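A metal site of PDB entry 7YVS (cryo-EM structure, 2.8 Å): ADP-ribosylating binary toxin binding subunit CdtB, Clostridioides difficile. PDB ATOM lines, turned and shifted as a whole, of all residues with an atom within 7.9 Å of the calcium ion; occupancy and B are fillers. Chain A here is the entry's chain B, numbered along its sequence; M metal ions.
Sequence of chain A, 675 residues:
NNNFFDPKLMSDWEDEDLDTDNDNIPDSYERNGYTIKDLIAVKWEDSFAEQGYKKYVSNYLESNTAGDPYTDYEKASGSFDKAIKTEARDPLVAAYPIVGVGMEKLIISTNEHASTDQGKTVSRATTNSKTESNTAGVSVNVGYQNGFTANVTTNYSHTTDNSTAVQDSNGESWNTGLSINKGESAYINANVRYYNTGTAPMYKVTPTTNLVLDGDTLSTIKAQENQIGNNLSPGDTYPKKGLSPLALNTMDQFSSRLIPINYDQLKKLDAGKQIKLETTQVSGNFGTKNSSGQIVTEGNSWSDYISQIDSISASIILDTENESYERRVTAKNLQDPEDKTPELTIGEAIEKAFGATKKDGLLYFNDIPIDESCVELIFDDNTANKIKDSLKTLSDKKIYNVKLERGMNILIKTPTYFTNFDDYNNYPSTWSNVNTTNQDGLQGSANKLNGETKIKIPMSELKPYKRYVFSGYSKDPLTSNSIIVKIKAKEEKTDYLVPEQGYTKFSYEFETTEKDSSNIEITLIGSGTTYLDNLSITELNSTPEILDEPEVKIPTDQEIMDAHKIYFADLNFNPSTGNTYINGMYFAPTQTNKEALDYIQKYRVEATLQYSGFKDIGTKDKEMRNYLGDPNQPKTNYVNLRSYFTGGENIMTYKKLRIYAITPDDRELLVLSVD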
ATOM      1  N   PHE A 418      13.807  31.138   0.239  1.00  0.00           N
ATOM      2  CA  PHE A 418      14.745  30.472  -0.648  1.00  0.00           C
ATOM      3  C   PHE A 418      14.341  29.021  -0.806  1.00  0.00           C
ATOM      4  O   PHE A 418      13.989  28.366   0.177  1.00  0.00           O
ATOM      5  CB  PHE A 418      16.181  30.579  -0.114  1.00  0.00           C
ATOM      6  CG  PHE A 418      17.154  29.665  -0.784  1.00  0.00           C
ATOM      7  CD1 PHE A 418      17.678  29.969  -2.020  1.00  0.00           C
ATOM      8  CD2 PHE A 418      17.557  28.480  -0.180  1.00  0.00           C
ATOM      9  CE1 PHE A 418      18.581  29.130  -2.638  1.00  0.00           C
ATOM     10  CE2 PHE A 418      18.456  27.637  -0.791  1.00  0.00           C
ATOM     11  CZ  PHE A 418      18.967  27.970  -2.029  1.00  0.00           C
ATOM     12  N   THR A 419      14.376  28.528  -2.041  1.00  0.00           N
ATOM     13  CA  THR A 419      14.090  27.131  -2.334  1.00  0.00           C
ATOM     14  C   THR A 419      15.148  26.579  -3.262  1.00  0.00           C
ATOM     15  O   THR A 419      15.547  27.242  -4.233  1.00  0.00           O
ATOM     16  CB  THR A 419      12.686  26.962  -2.939  1.00  0.00           C
ATOM     17  OG1 THR A 419      12.426  25.573  -3.175  1.00  0.00           O
ATOM     18  CG2 THR A 419      12.539  27.736  -4.242  1.00  0.00           C
ATOM     19  N   ASN A 420      15.626  25.375  -2.961  1.00  0.00           N
ATOM     20  CA  ASN A 420      16.633  24.707  -3.767  1.00  0.00           C
ATOM     21  C   ASN A 420      16.094  23.471  -4.469  1.00  0.00           C
ATOM     22  O   ASN A 420      16.817  22.847  -5.249  1.00  0.00           O
ATOM     23  CB  ASN A 420      17.832  24.319  -2.899  1.00  0.00           C
ATOM     24  CG  ASN A 420      17.431  23.524  -1.676  1.00  0.00           C
ATOM     25  OD1 ASN A 420      16.256  23.459  -1.333  1.00  0.00           O
ATOM     26  ND2 ASN A 420      18.411  22.912  -1.022  1.00  0.00           N
ATOM     27  N   PHE A 421      14.834  23.102  -4.211  1.00  0.00           N
ATOM     28  CA  PHE A 421      14.151  21.942  -4.769  1.00  0.00           C
ATOM     29  C   PHE A 421      14.709  20.619  -4.277  1.00  0.00           C
ATOM     30  O   PHE A 421      14.446  19.577  -4.897  1.00  0.00           O
ATOM     31  CB  PHE A 421      14.163  21.969  -6.309  1.00  0.00           C
ATOM     32  CG  PHE A 421      13.675  23.252  -6.898  1.00  0.00           C
ATOM     33  CD1 PHE A 421      12.475  23.803  -6.485  1.00  0.00           C
ATOM     34  CD2 PHE A 421      14.416  23.919  -7.856  1.00  0.00           C
ATOM     35  CE1 PHE A 421      12.011  24.992  -7.026  1.00  0.00           C
ATOM     36  CE2 PHE A 421      13.964  25.105  -8.406  1.00  0.00           C
ATOM     37  CZ  PHE A 421      12.764  25.644  -7.987  1.00  0.00           C
ATOM     38  N   ASP A 422      15.473  20.616  -3.182  1.00  0.00           N
ATOM     39  CA  ASP A 422      15.887  19.369  -2.546  1.00  0.00           C
ATOM     40  C   ASP A 422      15.297  19.212  -1.153  1.00  0.00           C
ATOM     41  O   ASP A 422      14.546  18.265  -0.906  1.00  0.00           O
ATOM     42  CB  ASP A 422      17.418  19.297  -2.455  1.00  0.00           C
ATOM     43  CG  ASP A 422      18.090  19.494  -3.798  1.00  0.00           C
ATOM     44  OD1 ASP A 422      18.082  20.631  -4.314  1.00  0.00           O
ATOM     45  OD2 ASP A 422      18.658  18.509  -4.329  1.00  0.00           O
ATOM     46  N   ASP A 423      15.614  20.117  -0.229  1.00  0.00           N
ATOM     47  CA  ASP A 423      15.138  19.987   1.140  1.00  0.00           C
ATOM     48  C   ASP A 423      14.669  21.281   1.785  1.00  0.00           C
ATOM     49  O   ASP A 423      14.019  21.214   2.831  1.00  0.00           O
ATOM     50  CB  ASP A 423      16.247  19.388   2.024  1.00  0.00           C
ATOM     51  CG  ASP A 423      17.537  20.164   1.935  1.00  0.00           C
ATOM     52  OD1 ASP A 423      17.638  21.051   1.063  1.00  0.00           O
ATOM     53  OD2 ASP A 423      18.449  19.902   2.742  1.00  0.00           O
ATOM     54  N   ASP A 440      19.350  17.195 -12.146  1.00  0.00           N
ATOM     55  CA  ASP A 440      20.101  18.283 -12.758  1.00  0.00           C
ATOM     56  C   ASP A 440      20.183  19.473 -11.802  1.00  0.00           C
ATOM     57  O   ASP A 440      19.845  19.349 -10.621  1.00  0.00           O
ATOM     58  CB  ASP A 440      19.452  18.701 -14.075  1.00  0.00           C
ATOM     59  CG  ASP A 440      20.456  19.268 -15.060  1.00  0.00           C
ATOM     60  OD1 ASP A 440      21.663  19.292 -14.723  1.00  0.00           O
ATOM     61  OD2 ASP A 440      20.052  19.688 -16.157  1.00  0.00           O
ATOM     62  N   GLY A 441      20.645  20.609 -12.301  1.00  0.00           N
ATOM     63  CA  GLY A 441      20.723  21.802 -11.494  1.00  0.00           C
ATOM     64  C   GLY A 441      22.038  21.926 -10.754  1.00  0.00           C
ATOM     65  O   GLY A 441      22.964  21.133 -10.900  1.00  0.00           O
ATOM     66  N   LEU A 442      22.122  22.980  -9.934  1.00  0.00           N
ATOM     67  CA  LEU A 442      23.350  23.256  -9.201  1.00  0.00           C
ATOM     68  C   LEU A 442      23.615  22.179  -8.154  1.00  0.00           C
ATOM     69  O   LEU A 442      24.736  21.673  -8.039  1.00  0.00           O
ATOM     70  CB  LEU A 442      23.277  24.636  -8.555  1.00  0.00           C
ATOM     71  CG  LEU A 442      23.838  25.770  -9.413  1.00  0.00           C
ATOM     72  CD1 LEU A 442      23.381  27.126  -8.902  1.00  0.00           C
ATOM     73  CD2 LEU A 442      25.355  25.701  -9.449  1.00  0.00           C
ATOM     74  N   GLN A 443      22.602  21.824  -7.365  1.00  0.00           N
ATOM     75  CA  GLN A 443      22.730  20.767  -6.364  1.00  0.00           C
ATOM     76  C   GLN A 443      21.572  19.787  -6.532  1.00  0.00           C
ATOM     77  O   GLN A 443      20.578  19.856  -5.806  1.00  0.00           O
ATOM     78  CB  GLN A 443      22.774  21.331  -4.937  1.00  0.00           C
ATOM     79  CG  GLN A 443      24.073  22.027  -4.544  1.00  0.00           C
ATOM     80  CD  GLN A 443      24.278  23.360  -5.216  1.00  0.00           C
ATOM     81  OE1 GLN A 443      25.261  23.563  -5.941  1.00  0.00           O
ATOM     82  NE2 GLN A 443      23.358  24.292  -4.984  1.00  0.00           N
ATOM     83  N   GLY A 444      21.716  18.874  -7.496  1.00  0.00           N
ATOM     84  CA  GLY A 444      20.872  17.696  -7.580  1.00  0.00           C
ATOM     85  C   GLY A 444      19.386  17.930  -7.670  1.00  0.00           C
ATOM     86  O   GLY A 444      18.609  17.085  -7.212  1.00  0.00           O
ATOM     87  N   SER A 445      18.958  19.050  -8.239  1.00  0.00           N
ATOM     88  CA  SER A 445      17.535  19.325  -8.414  1.00  0.00           C
ATOM     89  C   SER A 445      17.383  20.514  -9.343  1.00  0.00           C
ATOM     90  O   SER A 445      18.115  21.499  -9.231  1.00  0.00           O
ATOM     91  CB  SER A 445      16.844  19.611  -7.073  1.00  0.00           C
ATOM     92  OG  SER A 445      17.356  20.784  -6.471  1.00  0.00           O
ATOM     93  N   ALA A 446      16.420  20.418 -10.267  1.00  0.00           N
ATOM     94  CA  ALA A 446      16.128  21.522 -11.178  1.00  0.00           C
ATOM     95  C   ALA A 446      14.686  22.003 -11.067  1.00  0.00           C
ATOM     96  O   ALA A 446      14.454  23.204 -10.941  1.00  0.00           O
ATOM     97  CB  ALA A 446      16.431  21.099 -12.614  1.00  0.00           C
ATOM     98  N   ASN A 447      13.724  21.094 -11.101  1.00  0.00           N
ATOM     99  CA  ASN A 447      12.307  21.422 -10.959  1.00  0.00           C
ATOM    100  C   ASN A 447      11.889  22.532 -11.932  1.00  0.00           C
ATOM    101  O   ASN A 447      11.420  23.596 -11.531  1.00  0.00           O
ATOM    102  CB  ASN A 447      11.971  21.807  -9.519  1.00  0.00           C
ATOM    103  CG  ASN A 447      10.480  21.764  -9.222  1.00  0.00           C
ATOM    104  OD1 ASN A 447       9.664  21.530 -10.114  1.00  0.00           O
ATOM    105  ND2 ASN A 447      10.122  21.979  -7.966  1.00  0.00           N
ATOM    106  N   TYR A 503      25.324  27.958 -15.800  1.00  0.00           N
ATOM    107  CA  TYR A 503      24.399  28.617 -14.894  1.00  0.00           C
ATOM    108  C   TYR A 503      24.877  30.030 -14.589  1.00  0.00           C
ATOM    109  O   TYR A 503      26.057  30.234 -14.294  1.00  0.00           O
ATOM    110  CB  TYR A 503      24.240  27.827 -13.601  1.00  0.00           C
ATOM    111  CG  TYR A 503      23.139  26.797 -13.629  1.00  0.00           C
ATOM    112  CD1 TYR A 503      21.811  27.173 -13.515  1.00  0.00           C
ATOM    113  CD2 TYR A 503      23.430  25.444 -13.726  1.00  0.00           C
ATOM    114  CE1 TYR A 503      20.799  26.236 -13.535  1.00  0.00           C
ATOM    115  CE2 TYR A 503      22.431  24.502 -13.741  1.00  0.00           C
ATOM    116  CZ  TYR A 503      21.112  24.902 -13.644  1.00  0.00           C
ATOM    117  OH  TYR A 503      20.107  23.969 -13.657  1.00  0.00           O
ATOM    118  N   LEU A 532      16.092  25.755 -13.946  1.00  0.00           N
ATOM    119  CA  LEU A 532      16.234  26.753 -12.888  1.00  0.00           C
ATOM    120  C   LEU A 532      16.667  26.060 -11.599  1.00  0.00           C
ATOM    121  O   LEU A 532      16.534  24.841 -11.451  1.00  0.00           O
ATOM    122  CB  LEU A 532      14.922  27.511 -12.649  1.00  0.00           C
ATOM    123  CG  LEU A 532      14.376  28.345 -13.808  1.00  0.00           C
ATOM    124  CD1 LEU A 532      13.032  28.948 -13.433  1.00  0.00           C
ATOM    125  CD2 LEU A 532      15.355  29.433 -14.199  1.00  0.00           C
ATOM    126  N   ASP A 533      17.214  26.848 -10.680  1.00  0.00           N
ATOM    127  CA  ASP A 533      17.640  26.340  -9.383  1.00  0.00           C
ATOM    128  C   ASP A 533      17.923  27.511  -8.451  1.00  0.00           C
ATOM    129  O   ASP A 533      18.303  28.599  -8.901  1.00  0.00           O
ATOM    130  CB  ASP A 533      18.883  25.454  -9.508  1.00  0.00           C
ATOM    131  CG  ASP A 533      18.917  24.354  -8.464  1.00  0.00           C
ATOM    132  OD1 ASP A 533      17.958  24.267  -7.658  1.00  0.00           O
ATOM    133  OD2 ASP A 533      19.893  23.579  -8.452  1.00  0.00           O
ATOM    134  N   ASN A 534      17.719  27.273  -7.154  1.00  0.00           N
ATOM    135  CA  ASN A 534      18.108  28.190  -6.090  1.00  0.00           C
ATOM    136  C   ASN A 534      17.474  29.568  -6.267  1.00  0.00           C
ATOM    137  O   ASN A 534      18.139  30.580  -6.469  1.00  0.00           O
ATOM    138  CB  ASN A 534      19.631  28.305  -6.004  1.00  0.00           C
ATOM    139  CG  ASN A 534      20.294  27.002  -5.595  1.00  0.00           C
ATOM    140  OD1 ASN A 534      19.616  26.025  -5.300  1.00  0.00           O
ATOM    141  ND2 ASN A 534      21.614  26.991  -5.587  1.00  0.00           N
ATOM    142  N   LEU A 535      16.141  29.590  -6.186  1.00  0.00           N
ATOM    143  CA  LEU A 535      15.403  30.841  -6.261  1.00  0.00           C
ATOM    144  C   LEU A 535      15.286  31.455  -4.872  1.00  0.00           C
ATOM    145  O   LEU A 535      14.939  30.770  -3.908  1.00  0.00           O
ATOM    146  CB  LEU A 535      14.014  30.606  -6.862  1.00  0.00           C
ATOM    147  CG  LEU A 535      13.976  29.974  -8.250  1.00  0.00           C
ATOM    148  CD1 LEU A 535      12.539  29.744  -8.690  1.00  0.00           C
ATOM    149  CD2 LEU A 535      14.723  30.835  -9.257  1.00  0.00           C
HETATM  150 CA    CA M   1      19.043  22.475  -6.358  1.00  0.00          CA
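OG of Ser 445 sits close to OD2 of Asp 422, 3.4 Å away.
The backbone carbonyl oxygen of Gln 443 sits close to the side-chain hydroxyl of Ser 445 (3.4 Å).
The backbone carbonyl oxygen (O) of Asp 440 lies within hydrogen-bond range of the backbone NH (N) of Ser 445 (2.6 Å).
The side-chain carboxylate of Asp 533 sits close to the backbone NH of Gln 443 (3.4 Å).
OD1 of Asp 533 lies close to OD1 of Asn 534, 3.4 Å away.
OD2 of Asp 533 sits close to N of Leu 442 (2.7 Å).
OD1 of Asn 420 sits close to N of Asp 422 (3.5 Å).
The side-chain amide nitrogen (ND2) of Asn 420 sits at hydrogen-bond distance from the side-chain carboxylate (OD1) of Asp 423 (2.9 Å).
Merely in contact with the calcium ion: Asn 534 (3.7 Å).
Along chain A the residues within 4 Å of the calcium ion span positions 420 to 534.
The nearest printed residue that does not touch the calcium ion is Gly 444 (4.6 Å).
OG of Ser 445 binds the calcium ion (2.4 Å).
The calcium ion is bound by the side-chain carboxylate (OD1) of Asp 533 (2.5 Å).
The calcium ion is bound by O of Asn 420 (2.5 Å).
The side-chain carboxylate (OD2) of Asp 533 binds the calcium ion.
The calcium ion has four donor atoms within binding distance.
Slightly farther from the calcium ion lies the side-chain carboxylate (OD1) of Asp 422 (2.9 Å).
Slightly farther from the calcium ion lies O of Gln 443 (3.1 Å).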
